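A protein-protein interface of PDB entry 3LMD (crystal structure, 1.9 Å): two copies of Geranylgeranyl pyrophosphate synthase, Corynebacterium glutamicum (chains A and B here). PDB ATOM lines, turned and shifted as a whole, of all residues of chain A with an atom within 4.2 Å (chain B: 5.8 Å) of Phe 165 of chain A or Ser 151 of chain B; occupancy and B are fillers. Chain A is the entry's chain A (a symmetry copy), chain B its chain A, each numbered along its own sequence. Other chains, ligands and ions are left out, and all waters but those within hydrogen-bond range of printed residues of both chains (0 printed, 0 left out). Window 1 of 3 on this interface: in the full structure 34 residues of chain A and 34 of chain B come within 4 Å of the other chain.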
ATOM      1  N   THR A 107     -16.862   5.939  18.265  1.00  0.00           N
ATOM      2  CA  THR A 107     -15.660   5.110  18.456  1.00  0.00           C
ATOM      3  C   THR A 107     -15.920   3.669  18.082  1.00  0.00           C
ATOM      4  O   THR A 107     -15.091   3.027  17.407  1.00  0.00           O
ATOM      5  CB  THR A 107     -15.174   5.203  19.906  1.00  0.00           C
ATOM      6  OG1 THR A 107     -14.807   6.569  20.168  1.00  0.00           O
ATOM      7  CG2 THR A 107     -13.938   4.293  20.134  1.00  0.00           C
ATOM      8  N   MET A 154     -15.142  15.494  22.207  1.00  0.00           N
ATOM      9  CA  MET A 154     -14.381  15.323  23.472  1.00  0.00           C
ATOM     10  C   MET A 154     -13.729  16.605  23.932  1.00  0.00           C
ATOM     11  O   MET A 154     -13.575  16.812  25.132  1.00  0.00           O
ATOM     12  CB  MET A 154     -13.276  14.227  23.315  1.00  0.00           C
ATOM     13  CG  MET A 154     -13.906  12.847  23.206  1.00  0.00           C
ATOM     14  SD  MET A 154     -12.647  11.506  23.404  1.00  0.00           S
ATOM     15  CE  MET A 154     -11.325  12.306  22.737  1.00  0.00           C
ATOM     16  N   THR A 161     -12.322  13.161  30.041  1.00  0.00           N
ATOM     17  CA  THR A 161     -12.949  12.312  29.016  1.00  0.00           C
ATOM     18  C   THR A 161     -11.902  11.890  28.008  1.00  0.00           C
ATOM     19  O   THR A 161     -11.858  10.715  27.564  1.00  0.00           O
ATOM     20  CB  THR A 161     -14.120  13.044  28.313  1.00  0.00           C
ATOM     21  OG1 THR A 161     -15.154  13.259  29.287  1.00  0.00           O
ATOM     22  CG2 THR A 161     -14.689  12.221  27.090  1.00  0.00           C
ATOM     23  N   VAL A 162     -11.042  12.833  27.651  1.00  0.00           N
ATOM     24  CA  VAL A 162      -9.993  12.562  26.662  1.00  0.00           C
ATOM     25  C   VAL A 162      -9.012  11.488  27.200  1.00  0.00           C
ATOM     26  O   VAL A 162      -8.610  10.589  26.476  1.00  0.00           O
ATOM     27  CB  VAL A 162      -9.213  13.844  26.274  1.00  0.00           C
ATOM     28  CG1 VAL A 162      -8.068  13.537  25.283  1.00  0.00           C
ATOM     29  CG2 VAL A 162     -10.178  14.905  25.630  1.00  0.00           C
ATOM     30  N   ALA A 163      -8.637  11.602  28.475  1.00  0.00           N
ATOM     31  CA  ALA A 163      -7.703  10.659  29.103  1.00  0.00           C
ATOM     32  C   ALA A 163      -8.332   9.277  29.112  1.00  0.00           C
ATOM     33  O   ALA A 163      -7.680   8.260  28.799  1.00  0.00           O
ATOM     34  CB  ALA A 163      -7.420  11.102  30.540  1.00  0.00           C
ATOM     35  N   HIS A 164      -9.612   9.228  29.480  1.00  0.00           N
ATOM     36  CA  HIS A 164     -10.335   7.961  29.515  1.00  0.00           C
ATOM     37  C   HIS A 164     -10.474   7.374  28.111  1.00  0.00           C
ATOM     38  O   HIS A 164     -10.304   6.169  27.909  1.00  0.00           O
ATOM     39  CB  HIS A 164     -11.712   8.150  30.151  1.00  0.00           C
ATOM     40  CG  HIS A 164     -12.566   6.935  30.074  1.00  0.00           C
ATOM     41  ND1 HIS A 164     -12.472   5.907  30.989  1.00  0.00           N
ATOM     42  CD2 HIS A 164     -13.495   6.550  29.161  1.00  0.00           C
ATOM     43  CE1 HIS A 164     -13.324   4.946  30.653  1.00  0.00           C
ATOM     44  NE2 HIS A 164     -13.954   5.314  29.549  1.00  0.00           N
ATOM     45  N   PHE A 165     -10.774   8.224  27.133  1.00  0.00           N
ATOM     46  CA  PHE A 165     -10.806   7.788  25.729  1.00  0.00           C
ATOM     47  C   PHE A 165      -9.465   7.205  25.294  1.00  0.00           C
ATOM     48  O   PHE A 165      -9.403   6.140  24.655  1.00  0.00           O
ATOM     49  CB  PHE A 165     -11.175   8.969  24.795  1.00  0.00           C
ATOM     50  CG  PHE A 165     -10.957   8.667  23.325  1.00  0.00           C
ATOM     51  CD1 PHE A 165     -11.935   8.015  22.587  1.00  0.00           C
ATOM     52  CD2 PHE A 165      -9.742   8.949  22.716  1.00  0.00           C
ATOM     53  CE1 PHE A 165     -11.716   7.717  21.228  1.00  0.00           C
ATOM     54  CE2 PHE A 165      -9.509   8.639  21.365  1.00  0.00           C
ATOM     55  CZ  PHE A 165     -10.505   8.006  20.622  1.00  0.00           C
ATOM     56  N   ALA A 166      -8.379   7.894  25.630  1.00  0.00           N
ATOM     57  CA  ALA A 166      -7.059   7.434  25.211  1.00  0.00           C
ATOM     58  C   ALA A 166      -6.810   5.996  25.697  1.00  0.00           C
ATOM     59  O   ALA A 166      -6.305   5.144  24.942  1.00  0.00           O
ATOM     60  CB  ALA A 166      -5.965   8.378  25.716  1.00  0.00           C
ATOM     61  N   GLU A 167      -7.195   5.724  26.943  1.00  0.00           N
ATOM     62  CA  GLU A 167      -7.020   4.396  27.530  1.00  0.00           C
ATOM     63  C   GLU A 167      -7.934   3.392  26.868  1.00  0.00           C
ATOM     64  O   GLU A 167      -7.507   2.309  26.472  1.00  0.00           O
ATOM     65  CB  GLU A 167      -7.323   4.415  29.033  1.00  0.00           C
ATOM     66  CG  GLU A 167      -7.066   3.054  29.673  1.00  0.00           C
ATOM     67  CD  GLU A 167      -7.363   3.005  31.166  1.00  0.00           C
ATOM     68  OE1 GLU A 167      -7.601   4.066  31.781  1.00  0.00           O
ATOM     69  OE2 GLU A 167      -7.343   1.883  31.722  1.00  0.00           O
ATOM     70  N   THR A 168      -9.216   3.742  26.768  1.00  0.00           N
ATOM     71  CA  THR A 168     -10.191   2.863  26.131  1.00  0.00           C
ATOM     72  C   THR A 168      -9.846   2.509  24.683  1.00  0.00           C
ATOM     73  O   THR A 168      -9.846   1.334  24.270  1.00  0.00           O
ATOM     74  CB  THR A 168     -11.595   3.525  26.176  1.00  0.00           C
ATOM     75  OG1 THR A 168     -11.941   3.742  27.558  1.00  0.00           O
ATOM     76  CG2 THR A 168     -12.604   2.638  25.513  1.00  0.00           C
ATOM     77  N   PHE A 169      -9.564   3.527  23.894  1.00  0.00           N
ATOM     78  CA  PHE A 169      -9.225   3.326  22.500  1.00  0.00           C
ATOM     79  C   PHE A 169      -7.902   2.535  22.349  1.00  0.00           C
ATOM     80  O   PHE A 169      -7.820   1.622  21.545  1.00  0.00           O
ATOM     81  CB  PHE A 169      -9.179   4.680  21.768  1.00  0.00           C
ATOM     82  CG  PHE A 169      -8.934   4.550  20.298  1.00  0.00           C
ATOM     83  CD1 PHE A 169      -9.774   3.772  19.511  1.00  0.00           C
ATOM     84  CD2 PHE A 169      -7.857   5.171  19.706  1.00  0.00           C
ATOM     85  CE1 PHE A 169      -9.549   3.632  18.154  1.00  0.00           C
ATOM     86  CE2 PHE A 169      -7.626   5.032  18.319  1.00  0.00           C
ATOM     87  CZ  PHE A 169      -8.473   4.250  17.564  1.00  0.00           C
ATOM     88  N   LEU B 146      -1.006   4.711  17.644  1.00  0.00           N
ATOM     89  CA  LEU B 146      -0.327   6.029  17.716  1.00  0.00           C
ATOM     90  C   LEU B 146      -1.310   7.148  18.052  1.00  0.00           C
ATOM     91  O   LEU B 146      -1.038   8.011  18.903  1.00  0.00           O
ATOM     92  CB  LEU B 146       0.481   6.334  16.428  1.00  0.00           C
ATOM     93  CG  LEU B 146       1.981   6.002  16.533  1.00  0.00           C
ATOM     94  CD1 LEU B 146       2.266   4.519  16.811  1.00  0.00           C
ATOM     95  CD2 LEU B 146       2.637   6.457  15.251  1.00  0.00           C
ATOM     96  N   LEU B 147      -2.467   7.132  17.406  1.00  0.00           N
ATOM     97  CA  LEU B 147      -3.524   8.117  17.726  1.00  0.00           C
ATOM     98  C   LEU B 147      -3.970   7.983  19.185  1.00  0.00           C
ATOM     99  O   LEU B 147      -4.202   8.986  19.864  1.00  0.00           O
ATOM    100  CB  LEU B 147      -4.724   7.998  16.742  1.00  0.00           C
ATOM    101  CG  LEU B 147      -4.241   8.295  15.294  1.00  0.00           C
ATOM    102  CD1 LEU B 147      -5.197   7.855  14.202  1.00  0.00           C
ATOM    103  CD2 LEU B 147      -3.856   9.789  15.074  1.00  0.00           C
ATOM    104  N   ALA B 148      -4.048   6.764  19.703  1.00  0.00           N
ATOM    105  CA  ALA B 148      -4.389   6.605  21.130  1.00  0.00           C
ATOM    106  C   ALA B 148      -3.285   7.211  22.030  1.00  0.00           C
ATOM    107  O   ALA B 148      -3.590   7.871  23.023  1.00  0.00           O
ATOM    108  CB  ALA B 148      -4.597   5.123  21.506  1.00  0.00           C
ATOM    109  N   HIS B 149      -2.018   6.945  21.708  1.00  0.00           N
ATOM    110  CA  HIS B 149      -0.888   7.574  22.432  1.00  0.00           C
ATOM    111  C   HIS B 149      -0.991   9.101  22.386  1.00  0.00           C
ATOM    112  O   HIS B 149      -0.805   9.796  23.405  1.00  0.00           O
ATOM    113  CB  HIS B 149       0.480   7.216  21.804  1.00  0.00           C
ATOM    114  CG  HIS B 149       0.826   5.758  21.875  1.00  0.00           C
ATOM    115  ND1 HIS B 149       0.487   4.969  22.940  1.00  0.00           N
ATOM    116  CD2 HIS B 149       1.525   4.968  21.027  1.00  0.00           C
ATOM    117  CE1 HIS B 149       0.939   3.741  22.746  1.00  0.00           C
ATOM    118  NE2 HIS B 149       1.568   3.716  21.582  1.00  0.00           N
ATOM    119  N   ALA B 150      -1.247   9.631  21.201  1.00  0.00           N
ATOM    120  CA  ALA B 150      -1.336  11.087  21.057  1.00  0.00           C
ATOM    121  C   ALA B 150      -2.457  11.647  21.942  1.00  0.00           C
ATOM    122  O   ALA B 150      -2.308  12.683  22.598  1.00  0.00           O
ATOM    123  CB  ALA B 150      -1.536  11.507  19.554  1.00  0.00           C
ATOM    124  N   SER B 151      -3.599  10.985  21.950  1.00  0.00           N
ATOM    125  CA  SER B 151      -4.714  11.447  22.787  1.00  0.00           C
ATOM    126  C   SER B 151      -4.359  11.447  24.268  1.00  0.00           C
ATOM    127  O   SER B 151      -4.788  12.346  25.013  1.00  0.00           O
ATOM    128  CB  SER B 151      -5.949  10.555  22.570  1.00  0.00           C
ATOM    129  OG  SER B 151      -6.329  10.608  21.212  1.00  0.00           O
ATOM    130  N   GLY B 152      -3.608  10.439  24.714  1.00  0.00           N
ATOM    131  CA  GLY B 152      -3.133  10.403  26.113  1.00  0.00           C
ATOM    132  C   GLY B 152      -2.379  11.688  26.453  1.00  0.00           C
ATOM    133  O   GLY B 152      -2.676  12.358  27.471  1.00  0.00           O
ATOM    134  N   LEU B 153      -1.404  12.048  25.614  1.00  0.00           N
ATOM    135  CA  LEU B 153      -0.627  13.289  25.852  1.00  0.00           C
ATOM    136  C   LEU B 153      -1.493  14.549  25.773  1.00  0.00           C
ATOM    137  O   LEU B 153      -1.356  15.487  26.576  1.00  0.00           O
ATOM    138  CB  LEU B 153       0.531  13.416  24.857  1.00  0.00           C
ATOM    139  CG  LEU B 153       1.654  12.382  24.988  1.00  0.00           C
ATOM    140  CD1 LEU B 153       2.692  12.610  23.872  1.00  0.00           C
ATOM    141  CD2 LEU B 153       2.294  12.487  26.400  1.00  0.00           C
ATOM    142  N   MET B 154      -2.382  14.594  24.796  1.00  0.00           N
ATOM    143  CA  MET B 154      -3.300  15.753  24.653  1.00  0.00           C
ATOM    144  C   MET B 154      -4.188  15.939  25.860  1.00  0.00           C
ATOM    145  O   MET B 154      -4.554  17.068  26.177  1.00  0.00           O
ATOM    146  CB  MET B 154      -4.204  15.596  23.386  1.00  0.00           C
ATOM    147  CG  MET B 154      -3.381  15.763  22.118  1.00  0.00           C
ATOM    148  SD  MET B 154      -4.458  15.966  20.628  1.00  0.00           S
ATOM    149  CE  MET B 154      -5.757  15.021  21.130  1.00  0.00           C
ATOM    150  N   SER B 155      -4.568  14.844  26.523  1.00  0.00           N
ATOM    151  CA  SER B 155      -5.361  14.953  27.758  1.00  0.00           C
ATOM    152  C   SER B 155      -4.630  15.749  28.838  1.00  0.00           C
ATOM    153  O   SER B 155      -5.256  16.301  29.744  1.00  0.00           O
ATOM    154  CB  SER B 155      -5.768  13.575  28.317  1.00  0.00           C
ATOM    155  OG  SER B 155      -4.693  12.901  29.019  1.00  0.00           O
ATOM    156  N   GLN B 156      -3.308  15.819  28.731  1.00  0.00           N
ATOM    157  CA  GLN B 156      -2.524  16.574  29.699  1.00  0.00           C
ATOM    158  C   GLN B 156      -2.251  17.989  29.193  1.00  0.00           C
ATOM    159  O   GLN B 156      -1.831  18.860  29.967  1.00  0.00           O
ATOM    160  CB  GLN B 156      -1.198  15.855  30.005  1.00  0.00           C
ATOM    161  CG  GLN B 156      -1.404  14.455  30.617  1.00  0.00           C
ATOM    162  CD  GLN B 156      -0.083  13.823  31.015  1.00  0.00           C
ATOM    163  OE1 GLN B 156       0.825  13.708  30.189  1.00  0.00           O
ATOM    164  NE2 GLN B 156       0.039  13.438  32.284  1.00  0.00           N
ATOM    165  N   PHE B 165      -6.423  19.812  17.540  1.00  0.00           N
ATOM    166  CA  PHE B 165      -6.110  18.498  16.957  1.00  0.00           C
ATOM    167  C   PHE B 165      -7.272  17.965  16.125  1.00  0.00           C
ATOM    168  O   PHE B 165      -7.087  17.474  14.998  1.00  0.00           O
ATOM    169  CB  PHE B 165      -5.766  17.473  18.067  1.00  0.00           C
ATOM    170  CG  PHE B 165      -5.707  16.041  17.570  1.00  0.00           C
ATOM    171  CD1 PHE B 165      -4.544  15.541  16.999  1.00  0.00           C
ATOM    172  CD2 PHE B 165      -6.838  15.238  17.586  1.00  0.00           C
ATOM    173  CE1 PHE B 165      -4.504  14.218  16.517  1.00  0.00           C
ATOM    174  CE2 PHE B 165      -6.812  13.922  17.092  1.00  0.00           C
ATOM    175  CZ  PHE B 165      -5.634  13.416  16.542  1.00  0.00           C
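2 positions are printed for both chains. Of the 8 pairs that touch across the chains among the printed residues, none has its exchanged pair printed and touching as well.
Of the printed residues of chain B, Phe 165 of chain A touches Ser 151. Of chain A, only Val 162, Phe 165 and Ala 166 come within 4 Å of Ser 151 of chain B. Printed residues of chain B within 4 Å of Ala 166 of chain A: Ala 148, Ser 151 and Gly 152. Printed residues of chain B within 4 Å of Ala 163 of chain A: Ser 155 (3.5 Å). Of the printed residues of chain A, Ala 148 of chain B touches Ala 166 and Phe 169. Of the printed residues of chain B, Phe 169 of chain A touches Ala 148 (3.7 Å). The nearest printed residue of chain B that does not touch Phe 165 of chain A is Ala 148 of chain B (5.5 Å). The nearest printed residue of chain A that does not touch Ser 151 of chain B is Ala 163 of chain A (5.2 Å).
Val 162 of chain A touches Ser 151 of chain B. Val 162 of chain A touches Ser 155 of chain B (CG1 to CB, 3.8 Å). Ser 155 of chain B touches Ala 163 of chain A. CE2 of Phe 165 of chain A touches OG of Ser 151 of chain B, 3.7 Å away. CB of Ala 166 of chain A touches O of Ala 148 of chain B, at 3.6 Å. Ala 166 of chain A touches Ser 151 of chain B. N of Gly 152 of chain B touches CB of Ala 166 of chain A (3.3 Å). Ala 148 of chain B touches Phe 169 of chain A (CB to CD2, 3.7 Å).
Of the 12 printed residues of chain B, 4 touch a printed residue of chain A. Hydrophobic or aromatic side chains of chain B within 4 Å of the printed part of chain A: Ala 148.
O of Gly 152 of chain B lies within hydrogen-bond range of OG of Ser 155 of chain B. OG of Ser 151 of chain B lies within hydrogen-bond range of O of Leu 147 of chain B (3.0 Å).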
